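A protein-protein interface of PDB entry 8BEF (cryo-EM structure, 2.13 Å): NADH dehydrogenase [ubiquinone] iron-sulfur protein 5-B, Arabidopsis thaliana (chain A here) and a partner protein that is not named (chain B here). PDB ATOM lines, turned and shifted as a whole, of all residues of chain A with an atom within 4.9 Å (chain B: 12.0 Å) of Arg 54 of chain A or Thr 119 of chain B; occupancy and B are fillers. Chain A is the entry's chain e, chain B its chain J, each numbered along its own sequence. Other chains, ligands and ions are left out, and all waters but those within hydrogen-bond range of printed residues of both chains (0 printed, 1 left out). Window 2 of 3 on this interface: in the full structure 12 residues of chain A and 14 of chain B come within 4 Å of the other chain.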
ATOM      1  N   GLU A  50      23.410 -29.178  16.415  1.00  0.00           N
ATOM      2  CA  GLU A  50      23.027 -27.769  16.426  1.00  0.00           C
ATOM      3  C   GLU A  50      24.143 -26.890  15.876  1.00  0.00           C
ATOM      4  O   GLU A  50      23.927 -26.073  14.968  1.00  0.00           O
ATOM      5  CB  GLU A  50      22.671 -27.348  17.855  1.00  0.00           C
ATOM      6  CG  GLU A  50      21.630 -26.248  17.965  1.00  0.00           C
ATOM      7  CD  GLU A  50      21.607 -25.599  19.340  1.00  0.00           C
ATOM      8  OE1 GLU A  50      21.284 -26.295  20.326  1.00  0.00           O
ATOM      9  OE2 GLU A  50      21.889 -24.389  19.437  1.00  0.00           O
ATOM     10  N   PHE A  51      25.353 -27.059  16.410  1.00  0.00           N
ATOM     11  CA  PHE A  51      26.480 -26.244  15.981  1.00  0.00           C
ATOM     12  C   PHE A  51      26.869 -26.557  14.541  1.00  0.00           C
ATOM     13  O   PHE A  51      27.261 -25.658  13.794  1.00  0.00           O
ATOM     14  CB  PHE A  51      27.664 -26.446  16.930  1.00  0.00           C
ATOM     15  CG  PHE A  51      27.444 -25.867  18.305  1.00  0.00           C
ATOM     16  CD1 PHE A  51      26.373 -25.028  18.553  1.00  0.00           C
ATOM     17  CD2 PHE A  51      28.310 -26.160  19.346  1.00  0.00           C
ATOM     18  CE1 PHE A  51      26.163 -24.498  19.807  1.00  0.00           C
ATOM     19  CE2 PHE A  51      28.106 -25.630  20.606  1.00  0.00           C
ATOM     20  CZ  PHE A  51      27.033 -24.799  20.838  1.00  0.00           C
ATOM     21  N   GLN A  52      26.756 -27.821  14.128  1.00  0.00           N
ATOM     22  CA  GLN A  52      27.041 -28.172  12.740  1.00  0.00           C
ATOM     23  C   GLN A  52      26.090 -27.461  11.781  1.00  0.00           C
ATOM     24  O   GLN A  52      26.516 -26.922  10.751  1.00  0.00           O
ATOM     25  CB  GLN A  52      26.947 -29.685  12.556  1.00  0.00           C
ATOM     26  CG  GLN A  52      27.344 -30.165  11.177  1.00  0.00           C
ATOM     27  CD  GLN A  52      28.086 -31.481  11.221  1.00  0.00           C
ATOM     28  OE1 GLN A  52      28.248 -32.082  12.281  1.00  0.00           O
ATOM     29  NE2 GLN A  52      28.558 -31.927  10.067  1.00  0.00           N
ATOM     30  N   ARG A  53      24.795 -27.450  12.103  1.00  0.00           N
ATOM     31  CA  ARG A  53      23.814 -26.776  11.255  1.00  0.00           C
ATOM     32  C   ARG A  53      24.061 -25.269  11.210  1.00  0.00           C
ATOM     33  O   ARG A  53      24.003 -24.640  10.140  1.00  0.00           O
ATOM     34  CB  ARG A  53      22.408 -27.094  11.763  1.00  0.00           C
ATOM     35  CG  ARG A  53      21.343 -26.082  11.400  1.00  0.00           C
ATOM     36  CD  ARG A  53      20.005 -26.494  11.986  1.00  0.00           C
ATOM     37  NE  ARG A  53      18.912 -25.670  11.488  1.00  0.00           N
ATOM     38  CZ  ARG A  53      18.180 -25.970  10.425  1.00  0.00           C
ATOM     39  NH1 ARG A  53      18.408 -27.065   9.718  1.00  0.00           N
ATOM     40  NH2 ARG A  53      17.199 -25.150  10.061  1.00  0.00           N
ATOM     41  N   ARG A  54      24.344 -24.666  12.368  1.00  0.00           N
ATOM     42  CA  ARG A  54      24.641 -23.238  12.380  1.00  0.00           C
ATOM     43  C   ARG A  54      25.909 -22.924  11.592  1.00  0.00           C
ATOM     44  O   ARG A  54      25.994 -21.879  10.933  1.00  0.00           O
ATOM     45  CB  ARG A  54      24.745 -22.734  13.819  1.00  0.00           C
ATOM     46  CG  ARG A  54      23.397 -22.358  14.403  1.00  0.00           C
ATOM     47  CD  ARG A  54      23.337 -22.501  15.916  1.00  0.00           C
ATOM     48  NE  ARG A  54      23.656 -21.256  16.603  1.00  0.00           N
ATOM     49  CZ  ARG A  54      23.632 -21.100  17.919  1.00  0.00           C
ATOM     50  NH1 ARG A  54      23.268 -22.082  18.727  1.00  0.00           N
ATOM     51  NH2 ARG A  54      23.980 -19.927  18.438  1.00  0.00           N
ATOM     52  N   ASN A  55      26.895 -23.823  11.628  1.00  0.00           N
ATOM     53  CA  ASN A  55      28.098 -23.631  10.830  1.00  0.00           C
ATOM     54  C   ASN A  55      27.804 -23.762   9.345  1.00  0.00           C
ATOM     55  O   ASN A  55      28.436 -23.086   8.535  1.00  0.00           O
ATOM     56  CB  ASN A  55      29.177 -24.624  11.250  1.00  0.00           C
ATOM     57  CG  ASN A  55      29.754 -24.313  12.620  1.00  0.00           C
ATOM     58  OD1 ASN A  55      29.552 -23.225  13.157  1.00  0.00           O
ATOM     59  ND2 ASN A  55      30.477 -25.267  13.188  1.00  0.00           N
ATOM     60  N   ARG A  56      26.864 -24.631   8.971  1.00  0.00           N
ATOM     61  CA  ARG A  56      26.416 -24.671   7.581  1.00  0.00           C
ATOM     62  C   ARG A  56      25.823 -23.332   7.161  1.00  0.00           C
ATOM     63  O   ARG A  56      26.077 -22.848   6.050  1.00  0.00           O
ATOM     64  CB  ARG A  56      25.394 -25.790   7.385  1.00  0.00           C
ATOM     65  CG  ARG A  56      25.942 -26.999   6.677  1.00  0.00           C
ATOM     66  CD  ARG A  56      24.903 -28.087   6.543  1.00  0.00           C
ATOM     67  NE  ARG A  56      25.375 -29.360   7.073  1.00  0.00           N
ATOM     68  CZ  ARG A  56      25.020 -29.858   8.247  1.00  0.00           C
ATOM     69  NH1 ARG A  56      24.174 -29.222   9.039  1.00  0.00           N
ATOM     70  NH2 ARG A  56      25.520 -31.028   8.633  1.00  0.00           N
ATOM     71  N   ILE A  57      25.029 -22.721   8.041  1.00  0.00           N
ATOM     72  CA  ILE A  57      24.454 -21.412   7.727  1.00  0.00           C
ATOM     73  C   ILE A  57      25.561 -20.381   7.530  1.00  0.00           C
ATOM     74  O   ILE A  57      25.552 -19.600   6.567  1.00  0.00           O
ATOM     75  CB  ILE A  57      23.466 -20.976   8.823  1.00  0.00           C
ATOM     76  CG1 ILE A  57      22.180 -21.794   8.740  1.00  0.00           C
ATOM     77  CG2 ILE A  57      23.152 -19.488   8.705  1.00  0.00           C
ATOM     78  CD1 ILE A  57      21.400 -21.813  10.028  1.00  0.00           C
ATOM     79  N   TYR A  58      26.539 -20.372   8.438  1.00  0.00           N
ATOM     80  CA  TYR A  58      27.666 -19.449   8.317  1.00  0.00           C
ATOM     81  C   TYR A  58      28.461 -19.705   7.039  1.00  0.00           C
ATOM     82  O   TYR A  58      28.925 -18.763   6.382  1.00  0.00           O
ATOM     83  CB  TYR A  58      28.563 -19.565   9.550  1.00  0.00           C
ATOM     84  CG  TYR A  58      29.991 -19.104   9.347  1.00  0.00           C
ATOM     85  CD1 TYR A  58      30.330 -17.762   9.438  1.00  0.00           C
ATOM     86  CD2 TYR A  58      31.001 -20.016   9.072  1.00  0.00           C
ATOM     87  CE1 TYR A  58      31.632 -17.341   9.257  1.00  0.00           C
ATOM     88  CE2 TYR A  58      32.305 -19.602   8.889  1.00  0.00           C
ATOM     89  CZ  TYR A  58      32.616 -18.269   8.982  1.00  0.00           C
ATOM     90  OH  TYR A  58      33.916 -17.860   8.800  1.00  0.00           O
ATOM     91  N   ILE B 110      31.698 -30.099  18.345  1.00  0.00           N
ATOM     92  CA  ILE B 110      32.048 -29.255  17.201  1.00  0.00           C
ATOM     93  C   ILE B 110      31.894 -27.792  17.605  1.00  0.00           C
ATOM     94  O   ILE B 110      30.830 -27.405  18.107  1.00  0.00           O
ATOM     95  CB  ILE B 110      31.168 -29.590  16.003  1.00  0.00           C
ATOM     96  CG1 ILE B 110      31.550 -30.958  15.438  1.00  0.00           C
ATOM     97  CG2 ILE B 110      31.290 -28.519  14.930  1.00  0.00           C
ATOM     98  CD1 ILE B 110      30.449 -31.635  14.696  1.00  0.00           C
ATOM     99  N   PRO B 111      32.914 -26.964  17.413  1.00  0.00           N
ATOM    100  CA  PRO B 111      32.812 -25.563  17.830  1.00  0.00           C
ATOM    101  C   PRO B 111      31.800 -24.786  17.003  1.00  0.00           C
ATOM    102  O   PRO B 111      31.566 -25.068  15.827  1.00  0.00           O
ATOM    103  CB  PRO B 111      34.230 -25.025  17.616  1.00  0.00           C
ATOM    104  CG  PRO B 111      34.815 -25.906  16.584  1.00  0.00           C
ATOM    105  CD  PRO B 111      34.216 -27.268  16.800  1.00  0.00           C
ATOM    106  N   LEU B 112      31.197 -23.793  17.647  1.00  0.00           N
ATOM    107  CA  LEU B 112      30.331 -22.846  16.960  1.00  0.00           C
ATOM    108  C   LEU B 112      31.187 -21.730  16.372  1.00  0.00           C
ATOM    109  O   LEU B 112      31.812 -20.968  17.115  1.00  0.00           O
ATOM    110  CB  LEU B 112      29.293 -22.286  17.929  1.00  0.00           C
ATOM    111  CG  LEU B 112      28.193 -21.397  17.354  1.00  0.00           C
ATOM    112  CD1 LEU B 112      27.245 -22.200  16.472  1.00  0.00           C
ATOM    113  CD2 LEU B 112      27.440 -20.701  18.473  1.00  0.00           C
ATOM    114  N   LEU B 113      31.223 -21.640  15.049  1.00  0.00           N
ATOM    115  CA  LEU B 113      32.000 -20.589  14.403  1.00  0.00           C
ATOM    116  C   LEU B 113      31.354 -19.233  14.666  1.00  0.00           C
ATOM    117  O   LEU B 113      30.155 -19.065  14.421  1.00  0.00           O
ATOM    118  CB  LEU B 113      32.117 -20.846  12.902  1.00  0.00           C
ATOM    119  CG  LEU B 113      32.636 -22.234  12.529  1.00  0.00           C
ATOM    120  CD1 LEU B 113      32.700 -22.419  11.027  1.00  0.00           C
ATOM    121  CD2 LEU B 113      34.001 -22.471  13.158  1.00  0.00           C
ATOM    122  N   PRO B 114      32.103 -18.250  15.164  1.00  0.00           N
ATOM    123  CA  PRO B 114      31.509 -16.939  15.469  1.00  0.00           C
ATOM    124  C   PRO B 114      31.238 -16.167  14.186  1.00  0.00           C
ATOM    125  O   PRO B 114      32.145 -15.927  13.388  1.00  0.00           O
ATOM    126  CB  PRO B 114      32.577 -16.259  16.331  1.00  0.00           C
ATOM    127  CG  PRO B 114      33.860 -16.881  15.892  1.00  0.00           C
ATOM    128  CD  PRO B 114      33.558 -18.271  15.394  1.00  0.00           C
ATOM    129  N   THR B 115      29.983 -15.782  13.995  1.00  0.00           N
ATOM    130  CA  THR B 115      29.529 -15.170  12.756  1.00  0.00           C
ATOM    131  C   THR B 115      29.479 -13.652  12.884  1.00  0.00           C
ATOM    132  O   THR B 115      29.605 -13.083  13.971  1.00  0.00           O
ATOM    133  CB  THR B 115      28.151 -15.713  12.365  1.00  0.00           C
ATOM    134  OG1 THR B 115      27.187 -15.338  13.357  1.00  0.00           O
ATOM    135  CG2 THR B 115      28.193 -17.225  12.260  1.00  0.00           C
ATOM    136  N   GLN B 116      29.291 -12.993  11.740  1.00  0.00           N
ATOM    137  CA  GLN B 116      29.145 -11.542  11.711  1.00  0.00           C
ATOM    138  C   GLN B 116      27.696 -11.159  11.978  1.00  0.00           C
ATOM    139  O   GLN B 116      27.095 -10.388  11.223  1.00  0.00           O
ATOM    140  CB  GLN B 116      29.613 -10.979  10.367  1.00  0.00           C
ATOM    141  CG  GLN B 116      31.051 -11.327  10.016  1.00  0.00           C
ATOM    142  CD  GLN B 116      32.055 -10.554  10.849  1.00  0.00           C
ATOM    143  OE1 GLN B 116      31.786  -9.437  11.287  1.00  0.00           O
ATOM    144  NE2 GLN B 116      33.222 -11.150  11.071  1.00  0.00           N
ATOM    145  N   ARG B 117      27.134 -11.700  13.054  1.00  0.00           N
ATOM    146  CA  ARG B 117      25.774 -11.410  13.474  1.00  0.00           C
ATOM    147  C   ARG B 117      25.725 -11.498  14.991  1.00  0.00           C
ATOM    148  O   ARG B 117      26.427 -12.308  15.601  1.00  0.00           O
ATOM    149  CB  ARG B 117      24.764 -12.372  12.848  1.00  0.00           C
ATOM    150  CG  ARG B 117      23.392 -11.769  12.610  1.00  0.00           C
ATOM    151  CD  ARG B 117      22.291 -12.771  12.905  1.00  0.00           C
ATOM    152  NE  ARG B 117      20.974 -12.238  12.582  1.00  0.00           N
ATOM    153  CZ  ARG B 117      20.126 -11.747  13.476  1.00  0.00           C
ATOM    154  NH1 ARG B 117      20.428 -11.704  14.763  1.00  0.00           N
ATOM    155  NH2 ARG B 117      18.948 -11.287  13.068  1.00  0.00           N
ATOM    156  N   ASN B 118      24.899 -10.652  15.594  1.00  0.00           N
ATOM    157  CA  ASN B 118      24.795 -10.605  17.048  1.00  0.00           C
ATOM    158  C   ASN B 118      23.898 -11.745  17.509  1.00  0.00           C
ATOM    159  O   ASN B 118      22.670 -11.627  17.515  1.00  0.00           O
ATOM    160  CB  ASN B 118      24.259  -9.255  17.506  1.00  0.00           C
ATOM    161  CG  ASN B 118      24.535  -8.990  18.969  1.00  0.00           C
ATOM    162  OD1 ASN B 118      25.582  -9.372  19.495  1.00  0.00           O
ATOM    163  ND2 ASN B 118      23.595  -8.335  19.642  1.00  0.00           N
ATOM    164  N   THR B 119      24.515 -12.859  17.900  1.00  0.00           N
ATOM    165  CA  THR B 119      23.783 -13.971  18.488  1.00  0.00           C
ATOM    166  C   THR B 119      23.438 -13.730  19.953  1.00  0.00           C
ATOM    167  O   THR B 119      22.647 -14.491  20.522  1.00  0.00           O
ATOM    168  CB  THR B 119      24.594 -15.264  18.351  1.00  0.00           C
ATOM    169  OG1 THR B 119      25.299 -15.255  17.104  1.00  0.00           O
ATOM    170  CG2 THR B 119      23.680 -16.483  18.383  1.00  0.00           C
ATOM    171  N   THR B 120      23.995 -12.682  20.567  1.00  0.00           N
ATOM    172  CA  THR B 120      23.743 -12.423  21.982  1.00  0.00           C
ATOM    173  C   THR B 120      22.263 -12.199  22.266  1.00  0.00           C
ATOM    174  O   THR B 120      21.796 -12.483  23.375  1.00  0.00           O
ATOM    175  CB  THR B 120      24.555 -11.215  22.451  1.00  0.00           C
ATOM    176  OG1 THR B 120      24.095 -10.037  21.778  1.00  0.00           O
ATOM    177  CG2 THR B 120      26.034 -11.419  22.157  1.00  0.00           C
ATOM    178  N   SER B 121      21.509 -11.710  21.282  1.00  0.00           N
ATOM    179  CA  SER B 121      20.085 -11.483  21.491  1.00  0.00           C
ATOM    180  C   SER B 121      19.299 -12.783  21.593  1.00  0.00           C
ATOM    181  O   SER B 121      18.171 -12.771  22.092  1.00  0.00           O
ATOM    182  CB  SER B 121      19.518 -10.625  20.363  1.00  0.00           C
ATOM    183  OG  SER B 121      18.979 -11.435  19.336  1.00  0.00           O
ATOM    184  N   LEU B 122      19.864 -13.898  21.139  1.00  0.00           N
ATOM    185  CA  LEU B 122      19.201 -15.190  21.229  1.00  0.00           C
ATOM    186  C   LEU B 122      19.463 -15.902  22.547  1.00  0.00           C
ATOM    187  O   LEU B 122      18.987 -17.025  22.732  1.00  0.00           O
ATOM    188  CB  LEU B 122      19.621 -16.082  20.057  1.00  0.00           C
ATOM    189  CG  LEU B 122      19.059 -15.650  18.700  1.00  0.00           C
ATOM    190  CD1 LEU B 122      19.113 -16.788  17.701  1.00  0.00           C
ATOM    191  CD2 LEU B 122      17.632 -15.153  18.856  1.00  0.00           C
ATOM    192  N   ARG B 123      20.209 -15.283  23.459  1.00  0.00           N
ATOM    193  CA  ARG B 123      20.362 -15.830  24.799  1.00  0.00           C
ATOM    194  C   ARG B 123      19.040 -15.709  25.547  1.00  0.00           C
ATOM    195  O   ARG B 123      18.525 -14.603  25.737  1.00  0.00           O
ATOM    196  CB  ARG B 123      21.477 -15.098  25.546  1.00  0.00           C
ATOM    197  CG  ARG B 123      22.426 -16.015  26.302  1.00  0.00           C
ATOM    198  CD  ARG B 123      23.835 -15.443  26.368  1.00  0.00           C
ATOM    199  NE  ARG B 123      24.545 -15.577  25.103  1.00  0.00           N
ATOM    200  CZ  ARG B 123      25.747 -15.070  24.860  1.00  0.00           C
ATOM    201  NH1 ARG B 123      26.409 -14.389  25.782  1.00  0.00           N
ATOM    202  NH2 ARG B 123      26.300 -15.252  23.664  1.00  0.00           N
ATOM    203  N   TYR B 124      18.484 -16.843  25.959  1.00  0.00           N
ATOM    204  CA  TYR B 124      17.221 -16.872  26.686  1.00  0.00           C
ATOM    205  C   TYR B 124      17.496 -16.872  28.185  1.00  0.00           C
ATOM    206  O   TYR B 124      18.289 -17.679  28.676  1.00  0.00           O
ATOM    207  CB  TYR B 124      16.406 -18.105  26.292  1.00  0.00           C
ATOM    208  CG  TYR B 124      15.046 -18.188  26.948  1.00  0.00           C
ATOM    209  CD1 TYR B 124      14.164 -17.114  26.903  1.00  0.00           C
ATOM    210  CD2 TYR B 124      14.644 -19.338  27.613  1.00  0.00           C
ATOM    211  CE1 TYR B 124      12.927 -17.184  27.498  1.00  0.00           C
ATOM    212  CE2 TYR B 124      13.406 -19.415  28.215  1.00  0.00           C
ATOM    213  CZ  TYR B 124      12.552 -18.336  28.155  1.00  0.00           C
ATOM    214  OH  TYR B 124      11.320 -18.411  28.752  1.00  0.00           O
ATOM    215  N   THR B 125      16.835 -15.972  28.908  1.00  0.00           N
ATOM    216  CA  THR B 125      17.027 -15.818  30.345  1.00  0.00           C
ATOM    217  C   THR B 125      15.839 -16.414  31.088  1.00  0.00           C
ATOM    218  O   THR B 125      14.690 -16.040  30.832  1.00  0.00           O
ATOM    219  CB  THR B 125      17.200 -14.346  30.721  1.00  0.00           C
ATOM    220  OG1 THR B 125      18.447 -13.866  30.203  1.00  0.00           O
ATOM    221  CG2 THR B 125      17.178 -14.169  32.227  1.00  0.00           C
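The guanidinium group (NH1) of Arg 54 of chain A lies within salt-bridge range of the side-chain carboxylate (OE2) of Glu 50 of chain A, at 2.8 Å.
O of Phe 51 of chain A sits close to ND2 of Asn 55 of chain A (3.3 Å).
NE2 of Gln 52 of chain A sits close to NH2 of Arg 56 of chain A, at 3.5 Å.
O of Arg 117 of chain B sits at hydrogen-bond distance from OG1 of Thr 119 of chain B, at 3.5 Å.
Of the 9 printed residues of chain A, 5 touch a printed residue of chain B.
Hydrophobic or aromatic side chains of chain A that line the printed part of chain B: Phe 51 and Tyr 58.
Hydrophobic or aromatic side chains of chain B within 4 Å of the printed part of chain A: Ile 110, Leu 112 and Leu 113.
Among the printed residues, 11 pairs touch across the chains.
Among the printed residues, no Asp or Glu carboxylate lies within 4 Å of a Lys or Arg side-chain nitrogen of the other chain.
Arg 54 of chain A touches two residues of chain B.
Of the printed residues of chain A, Thr 119 of chain B touches Arg 54 (3.5 Å).
No residue of chain B comes within 4 Å of Glu 50 of chain A.
Phe 51 of chain A touches just these residues of chain B: Ile 110 (3.1 Å) and Leu 112 (3.6 Å).
Asn 55 of chain A touches just these residues of chain B: Ile 110 (3.8 Å), Pro 111 (2.9 Å), Leu 112 (3.9 Å) and Leu 113 (3.0 Å).
No residue of chain B comes within 4 Å of Ile 57 of chain A.
Printed residues of chain A within 4 Å of Thr 115 of chain B: Tyr 58.
Printed residues of chain B within 4 Å of Tyr 58 of chain A: Leu 113 and Thr 115.
Of the printed residues of chain A, Pro 111 of chain B touches Asn 55 (2.9 Å).
Of the printed residues of chain A, Ile 110 of chain B touches Phe 51 (3.1 Å), Gln 52 (3.3 Å) and Asn 55 (3.8 Å).
The nearest printed residue of chain A that does not touch Thr 119 of chain B is Glu 50 of chain A (8.2 Å).
The nearest printed residue of chain A that does not touch Ile 110 of chain B is Glu 50 of chain A (7.1 Å).
Among the printed residues, merely in contact across the chains: Phe 51 of chain A with Ile 110 of chain B, Gln 52 of chain A with Ile 110 of chain B, Arg 54 of chain A with Thr 119 of chain B, Tyr 58 of chain A with Leu 113 of chain B, Arg 54 of chain A with Leu 112 of chain B, Tyr 58 of chain A with Thr 115 of chain B, Phe 51 of chain A with Leu 112 of chain B, Asn 55 of chain A with Ile 110 of chain B and Asn 55 of chain A with Leu 112 of chain B.
The side-chain amide nitrogen (ND2) of Asn 55 of chain A lies within hydrogen-bond range of the backbone carbonyl oxygen (O) of Pro 111 of chain B.
The side-chain amide oxygen (OD1) of Asn 55 of chain A lies within hydrogen-bond range of the backbone NH (N) of Leu 113 of chain B, at 3.0 Å.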
